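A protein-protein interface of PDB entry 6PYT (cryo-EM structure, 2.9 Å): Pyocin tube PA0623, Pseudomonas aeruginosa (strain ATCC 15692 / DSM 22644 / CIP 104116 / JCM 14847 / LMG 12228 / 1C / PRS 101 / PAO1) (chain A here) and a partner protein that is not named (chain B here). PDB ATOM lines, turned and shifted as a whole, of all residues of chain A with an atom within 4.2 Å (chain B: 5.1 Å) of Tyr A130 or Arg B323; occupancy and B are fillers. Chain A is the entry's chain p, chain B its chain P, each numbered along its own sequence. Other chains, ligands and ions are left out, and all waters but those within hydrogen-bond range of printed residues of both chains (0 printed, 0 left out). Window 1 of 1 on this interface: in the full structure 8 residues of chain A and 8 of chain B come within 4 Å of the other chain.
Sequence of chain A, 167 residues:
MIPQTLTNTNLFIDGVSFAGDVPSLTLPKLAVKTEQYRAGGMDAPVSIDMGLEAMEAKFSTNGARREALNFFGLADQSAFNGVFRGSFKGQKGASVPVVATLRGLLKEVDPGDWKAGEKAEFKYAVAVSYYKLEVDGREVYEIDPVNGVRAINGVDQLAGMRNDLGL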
ATOM      1  N   LEU A 102      14.803  -3.200  18.352  1.00  0.00           N
ATOM      2  CA  LEU A 102      13.661  -3.582  19.152  1.00  0.00           C
ATOM      3  C   LEU A 102      12.629  -4.266  18.274  1.00  0.00           C
ATOM      4  O   LEU A 102      12.630  -4.136  17.052  1.00  0.00           O
ATOM      5  CB  LEU A 102      13.073  -2.378  19.901  1.00  0.00           C
ATOM      6  CG  LEU A 102      12.533  -1.134  19.207  1.00  0.00           C
ATOM      7  CD1 LEU A 102      11.054  -1.256  18.915  1.00  0.00           C
ATOM      8  CD2 LEU A 102      12.802   0.066  20.073  1.00  0.00           C
ATOM      9  N   ARG A 103      11.736  -4.987  18.932  1.00  0.00           N
ATOM     10  CA  ARG A 103      10.820  -5.884  18.259  1.00  0.00           C
ATOM     11  C   ARG A 103       9.536  -5.940  19.067  1.00  0.00           C
ATOM     12  O   ARG A 103       9.581  -5.950  20.296  1.00  0.00           O
ATOM     13  CB  ARG A 103      11.464  -7.258  18.114  1.00  0.00           C
ATOM     14  CG  ARG A 103      10.686  -8.267  17.338  1.00  0.00           C
ATOM     15  CD  ARG A 103      11.531  -9.505  17.164  1.00  0.00           C
ATOM     16  NE  ARG A 103      12.683  -9.219  16.324  1.00  0.00           N
ATOM     17  CZ  ARG A 103      12.679  -9.310  15.001  1.00  0.00           C
ATOM     18  NH1 ARG A 103      11.587  -9.708  14.364  1.00  0.00           N
ATOM     19  NH2 ARG A 103      13.777  -9.028  14.318  1.00  0.00           N
ATOM     20  N   VAL A 128       6.781  -3.266  23.049  1.00  0.00           N
ATOM     21  CA  VAL A 128       8.108  -3.829  22.832  1.00  0.00           C
ATOM     22  C   VAL A 128       8.201  -5.224  23.439  1.00  0.00           C
ATOM     23  O   VAL A 128       8.039  -5.403  24.647  1.00  0.00           O
ATOM     24  CB  VAL A 128       9.183  -2.899  23.403  1.00  0.00           C
ATOM     25  CG1 VAL A 128      10.522  -3.518  23.280  1.00  0.00           C
ATOM     26  CG2 VAL A 128       9.165  -1.596  22.666  1.00  0.00           C
ATOM     27  N   SER A 129       8.471  -6.214  22.590  1.00  0.00           N
ATOM     28  CA  SER A 129       8.613  -7.604  22.987  1.00  0.00           C
ATOM     29  C   SER A 129      10.059  -8.066  23.018  1.00  0.00           C
ATOM     30  O   SER A 129      10.323  -9.198  23.424  1.00  0.00           O
ATOM     31  CB  SER A 129       7.828  -8.500  22.034  1.00  0.00           C
ATOM     32  OG  SER A 129       8.038  -9.859  22.350  1.00  0.00           O
ATOM     33  N   TYR A 130      10.986  -7.235  22.566  1.00  0.00           N
ATOM     34  CA  TYR A 130      12.413  -7.497  22.631  1.00  0.00           C
ATOM     35  C   TYR A 130      13.110  -6.162  22.522  1.00  0.00           C
ATOM     36  O   TYR A 130      12.722  -5.333  21.709  1.00  0.00           O
ATOM     37  CB  TYR A 130      12.898  -8.416  21.513  1.00  0.00           C
ATOM     38  CG  TYR A 130      14.393  -8.607  21.531  1.00  0.00           C
ATOM     39  CD1 TYR A 130      14.988  -9.411  22.481  1.00  0.00           C
ATOM     40  CD2 TYR A 130      15.210  -7.969  20.605  1.00  0.00           C
ATOM     41  CE1 TYR A 130      16.344  -9.584  22.508  1.00  0.00           C
ATOM     42  CE2 TYR A 130      16.566  -8.136  20.629  1.00  0.00           C
ATOM     43  CZ  TYR A 130      17.127  -8.945  21.582  1.00  0.00           C
ATOM     44  OH  TYR A 130      18.485  -9.125  21.611  1.00  0.00           O
ATOM     45  N   TYR A 131      14.146  -5.961  23.320  1.00  0.00           N
ATOM     46  CA  TYR A 131      14.813  -4.671  23.319  1.00  0.00           C
ATOM     47  C   TYR A 131      16.285  -4.859  23.623  1.00  0.00           C
ATOM     48  O   TYR A 131      16.630  -5.406  24.669  1.00  0.00           O
ATOM     49  CB  TYR A 131      14.167  -3.737  24.332  1.00  0.00           C
ATOM     50  CG  TYR A 131      14.839  -2.404  24.428  1.00  0.00           C
ATOM     51  CD1 TYR A 131      14.811  -1.516  23.369  1.00  0.00           C
ATOM     52  CD2 TYR A 131      15.471  -2.015  25.590  1.00  0.00           C
ATOM     53  CE1 TYR A 131      15.425  -0.296  23.457  1.00  0.00           C
ATOM     54  CE2 TYR A 131      16.085  -0.805  25.681  1.00  0.00           C
ATOM     55  CZ  TYR A 131      16.049   0.056  24.626  1.00  0.00           C
ATOM     56  OH  TYR A 131      16.663   1.271  24.745  1.00  0.00           O
ATOM     57  N   LYS A 132      17.143  -4.414  22.713  1.00  0.00           N
ATOM     58  CA  LYS A 132      18.579  -4.406  22.939  1.00  0.00           C
ATOM     59  C   LYS A 132      19.112  -3.014  22.663  1.00  0.00           C
ATOM     60  O   LYS A 132      18.972  -2.508  21.551  1.00  0.00           O
ATOM     61  CB  LYS A 132      19.303  -5.425  22.062  1.00  0.00           C
ATOM     62  CG  LYS A 132      20.784  -5.469  22.354  1.00  0.00           C
ATOM     63  CD  LYS A 132      21.499  -6.587  21.648  1.00  0.00           C
ATOM     64  CE  LYS A 132      21.727  -6.265  20.201  1.00  0.00           C
ATOM     65  NZ  LYS A 132      22.565  -7.316  19.576  1.00  0.00           N
ATOM     66  N   ILE A 143      16.664  -7.071  26.769  1.00  0.00           N
ATOM     67  CA  ILE A 143      15.470  -7.466  27.502  1.00  0.00           C
ATOM     68  C   ILE A 143      14.599  -8.286  26.575  1.00  0.00           C
ATOM     69  O   ILE A 143      14.121  -7.782  25.555  1.00  0.00           O
ATOM     70  CB  ILE A 143      14.685  -6.268  28.055  1.00  0.00           C
ATOM     71  CG1 ILE A 143      15.494  -5.517  29.103  1.00  0.00           C
ATOM     72  CG2 ILE A 143      13.411  -6.746  28.691  1.00  0.00           C
ATOM     73  CD1 ILE A 143      16.249  -4.359  28.576  1.00  0.00           C
ATOM     74  N   ASP A 144      14.392  -9.544  26.933  1.00  0.00           N
ATOM     75  CA  ASP A 144      13.521 -10.446  26.192  1.00  0.00           C
ATOM     76  C   ASP A 144      12.613 -11.082  27.232  1.00  0.00           C
ATOM     77  O   ASP A 144      13.070 -11.960  27.984  1.00  0.00           O
ATOM     78  CB  ASP A 144      14.332 -11.488  25.438  1.00  0.00           C
ATOM     79  N   ASN A 147      11.461 -16.115  27.082  1.00  0.00           N
ATOM     80  CA  ASN A 147      12.874 -16.470  27.264  1.00  0.00           C
ATOM     81  C   ASN A 147      13.549 -15.434  28.156  1.00  0.00           C
ATOM     82  O   ASN A 147      14.341 -14.623  27.690  1.00  0.00           O
ATOM     83  CB  ASN A 147      13.670 -16.595  25.956  1.00  0.00           C
ATOM     84  CG  ASN A 147      13.294 -17.792  25.146  1.00  0.00           C
ATOM     85  OD1 ASN A 147      13.084 -18.883  25.674  1.00  0.00           O
ATOM     86  ND2 ASN A 147      13.225 -17.604  23.838  1.00  0.00           N
ATOM     87  N   ARG B 319      18.954 -13.705  14.920  1.00  0.00           N
ATOM     88  CA  ARG B 319      18.770 -13.904  16.355  1.00  0.00           C
ATOM     89  C   ARG B 319      17.299 -13.991  16.732  1.00  0.00           C
ATOM     90  O   ARG B 319      16.952 -14.655  17.710  1.00  0.00           O
ATOM     91  CB  ARG B 319      19.426 -12.777  17.145  1.00  0.00           C
ATOM     92  CG  ARG B 319      20.931 -12.728  17.097  1.00  0.00           C
ATOM     93  CD  ARG B 319      21.440 -11.642  18.019  1.00  0.00           C
ATOM     94  NE  ARG B 319      22.892 -11.524  17.996  1.00  0.00           N
ATOM     95  CZ  ARG B 319      23.555 -10.594  17.324  1.00  0.00           C
ATOM     96  NH1 ARG B 319      22.896  -9.675  16.648  1.00  0.00           N
ATOM     97  NH2 ARG B 319      24.874 -10.565  17.355  1.00  0.00           N
ATOM     98  N   ALA B 320      16.423 -13.338  15.975  1.00  0.00           N
ATOM     99  CA  ALA B 320      15.007 -13.344  16.311  1.00  0.00           C
ATOM    100  C   ALA B 320      14.338 -14.652  15.923  1.00  0.00           C
ATOM    101  O   ALA B 320      13.462 -15.139  16.641  1.00  0.00           O
ATOM    102  CB  ALA B 320      14.306 -12.177  15.633  1.00  0.00           C
ATOM    103  N   PHE B 321      14.730 -15.235  14.796  1.00  0.00           N
ATOM    104  CA  PHE B 321      14.243 -16.549  14.400  1.00  0.00           C
ATOM    105  C   PHE B 321      15.051 -17.676  15.010  1.00  0.00           C
ATOM    106  O   PHE B 321      14.941 -18.814  14.557  1.00  0.00           O
ATOM    107  CB  PHE B 321      14.226 -16.675  12.876  1.00  0.00           C
ATOM    108  CG  PHE B 321      13.132 -15.885  12.226  1.00  0.00           C
ATOM    109  CD1 PHE B 321      11.843 -16.392  12.162  1.00  0.00           C
ATOM    110  CD2 PHE B 321      13.379 -14.624  11.704  1.00  0.00           C
ATOM    111  CE1 PHE B 321      10.818 -15.663  11.575  1.00  0.00           C
ATOM    112  CE2 PHE B 321      12.363 -13.886  11.115  1.00  0.00           C
ATOM    113  CZ  PHE B 321      11.079 -14.407  11.050  1.00  0.00           C
ATOM    114  N   MET B 322      15.855 -17.378  16.022  1.00  0.00           N
ATOM    115  CA  MET B 322      16.622 -18.359  16.761  1.00  0.00           C
ATOM    116  C   MET B 322      16.288 -18.342  18.240  1.00  0.00           C
ATOM    117  O   MET B 322      16.508 -19.347  18.918  1.00  0.00           O
ATOM    118  CB  MET B 322      18.120 -18.083  16.577  1.00  0.00           C
ATOM    119  CG  MET B 322      19.069 -19.192  16.829  1.00  0.00           C
ATOM    120  SD  MET B 322      19.079 -20.488  15.604  1.00  0.00           S
ATOM    121  CE  MET B 322      19.896 -21.733  16.576  1.00  0.00           C
ATOM    122  N   ARG B 323      15.772 -17.227  18.756  1.00  0.00           N
ATOM    123  CA  ARG B 323      15.175 -17.199  20.081  1.00  0.00           C
ATOM    124  C   ARG B 323      13.757 -17.748  20.075  1.00  0.00           C
ATOM    125  O   ARG B 323      13.211 -18.021  21.145  1.00  0.00           O
ATOM    126  CB  ARG B 323      15.170 -15.773  20.629  1.00  0.00           C
ATOM    127  CG  ARG B 323      14.134 -14.872  19.974  1.00  0.00           C
ATOM    128  CD  ARG B 323      14.172 -13.438  20.494  1.00  0.00           C
ATOM    129  NE  ARG B 323      15.319 -12.691  19.999  1.00  0.00           N
ATOM    130  CZ  ARG B 323      16.405 -12.463  20.714  1.00  0.00           C
ATOM    131  NH1 ARG B 323      16.491 -12.951  21.939  1.00  0.00           N
ATOM    132  NH2 ARG B 323      17.405 -11.771  20.199  1.00  0.00           N
ATOM    133  N   ASP B 324      13.146 -17.886  18.896  1.00  0.00           N
ATOM    134  CA  ASP B 324      11.911 -18.647  18.765  1.00  0.00           C
ATOM    135  C   ASP B 324      12.200 -20.139  18.868  1.00  0.00           C
ATOM    136  O   ASP B 324      11.329 -20.930  19.238  1.00  0.00           O
ATOM    137  CB  ASP B 324      11.241 -18.312  17.428  1.00  0.00           C
ATOM    138  N   LEU B 325      13.427 -20.537  18.542  1.00  0.00           N
ATOM    139  CA  LEU B 325      13.811 -21.936  18.639  1.00  0.00           C
ATOM    140  C   LEU B 325      14.295 -22.282  20.034  1.00  0.00           C
ATOM    141  O   LEU B 325      14.109 -23.412  20.495  1.00  0.00           O
ATOM    142  CB  LEU B 325      14.878 -22.236  17.599  1.00  0.00           C
ATOM    143  CG  LEU B 325      14.264 -22.185  16.212  1.00  0.00           C
ATOM    144  CD1 LEU B 325      15.334 -22.046  15.186  1.00  0.00           C
ATOM    145  CD2 LEU B 325      13.512 -23.466  15.981  1.00  0.00           C
ATOM    146  N   LYS B 326      14.916 -21.327  20.726  1.00  0.00           N
ATOM    147  CA  LYS B 326      15.278 -21.563  22.118  1.00  0.00           C
ATOM    148  C   LYS B 326      14.040 -21.539  23.000  1.00  0.00           C
ATOM    149  O   LYS B 326      14.007 -22.186  24.053  1.00  0.00           O
ATOM    150  CB  LYS B 326      16.298 -20.523  22.582  1.00  0.00           C
ATOM    151  CG  LYS B 326      16.903 -20.816  23.942  1.00  0.00           C
ATOM    152  CD  LYS B 326      17.949 -19.817  24.349  1.00  0.00           C
ATOM    153  CE  LYS B 326      17.326 -18.534  24.839  1.00  0.00           C
ATOM    154  NZ  LYS B 326      18.361 -17.607  25.378  1.00  0.00           N
ATOM    155  N   ASN B 327      13.002 -20.820  22.566  1.00  0.00           N
ATOM    156  CA  ASN B 327      11.768 -20.738  23.337  1.00  0.00           C
ATOM    157  C   ASN B 327      11.051 -22.077  23.371  1.00  0.00           C
ATOM    158  O   ASN B 327      10.638 -22.542  24.438  1.00  0.00           O
ATOM    159  CB  ASN B 327      10.845 -19.681  22.747  1.00  0.00           C
ATOM    160  CG  ASN B 327       9.765 -19.259  23.706  1.00  0.00           C
ATOM    161  OD1 ASN B 327       9.756 -19.662  24.865  1.00  0.00           O
ATOM    162  ND2 ASN B 327       8.826 -18.465  23.220  1.00  0.00           N
ATOM    163  N   PHE B 334      21.831 -20.377  21.887  1.00  0.00           N
ATOM    164  CA  PHE B 334      22.496 -20.130  20.610  1.00  0.00           C
ATOM    165  C   PHE B 334      23.521 -18.997  20.633  1.00  0.00           C
ATOM    166  O   PHE B 334      23.671 -18.285  21.628  1.00  0.00           O
ATOM    167  CB  PHE B 334      21.445 -19.788  19.554  1.00  0.00           C
ATOM    168  CG  PHE B 334      20.743 -18.469  19.799  1.00  0.00           C
ATOM    169  CD1 PHE B 334      19.672 -18.391  20.667  1.00  0.00           C
ATOM    170  CD2 PHE B 334      21.122 -17.320  19.118  1.00  0.00           C
ATOM    171  CE1 PHE B 334      19.035 -17.202  20.893  1.00  0.00           C
ATOM    172  CE2 PHE B 334      20.482 -16.130  19.341  1.00  0.00           C
ATOM    173  CZ  PHE B 334      19.435 -16.072  20.223  1.00  0.00           C
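Hydrophobic or aromatic side chains of chain A within 4 Å of the printed part of chain B: Tyr A130.
Printed residues of chain B within 4 Å of Arg A103: Ala B320. Of the printed residues of chain B, Tyr A130 touches Arg B323. Printed residues of chain A within 4 Å of Ala B320: Arg A103 (3.4 Å). Arg B323 touches just these residues of chain A: Tyr A130 and Asn A147. Of the printed residues of chain A, Asn B327 touches Asn A147. Phe B334 touches none of the printed residues of chain A. The nearest printed residue of chain B that does not touch Tyr A130 is Arg B319 (5.3 Å). The nearest printed residue of chain A that does not touch Arg B323 is Asp A144 (4.4 Å).
Among the printed residues, merely in contact across the chains: Arg A103 with Ala B320, Lys A132 with Arg B319 and Asn A147 with Lys B326.
O of Arg A103 is in hydrogen-bond range of N of Ser A129 (2.6 Å). The backbone NH of Tyr A130 is in hydrogen-bond range of the backbone carbonyl oxygen of Arg A103. The backbone carbonyl oxygen of Arg B319 sits at hydrogen-bond distance from the guanidinium group of Arg B323.
NH2 of Arg B323 sits close to OH of Tyr A130 (3.2 Å). ND2 of Asn A147 is in hydrogen-bond range of O of Arg B323, 2.7 Å away. ND2 of Asn A147 lies close to N of Asn B327 (3.5 Å).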
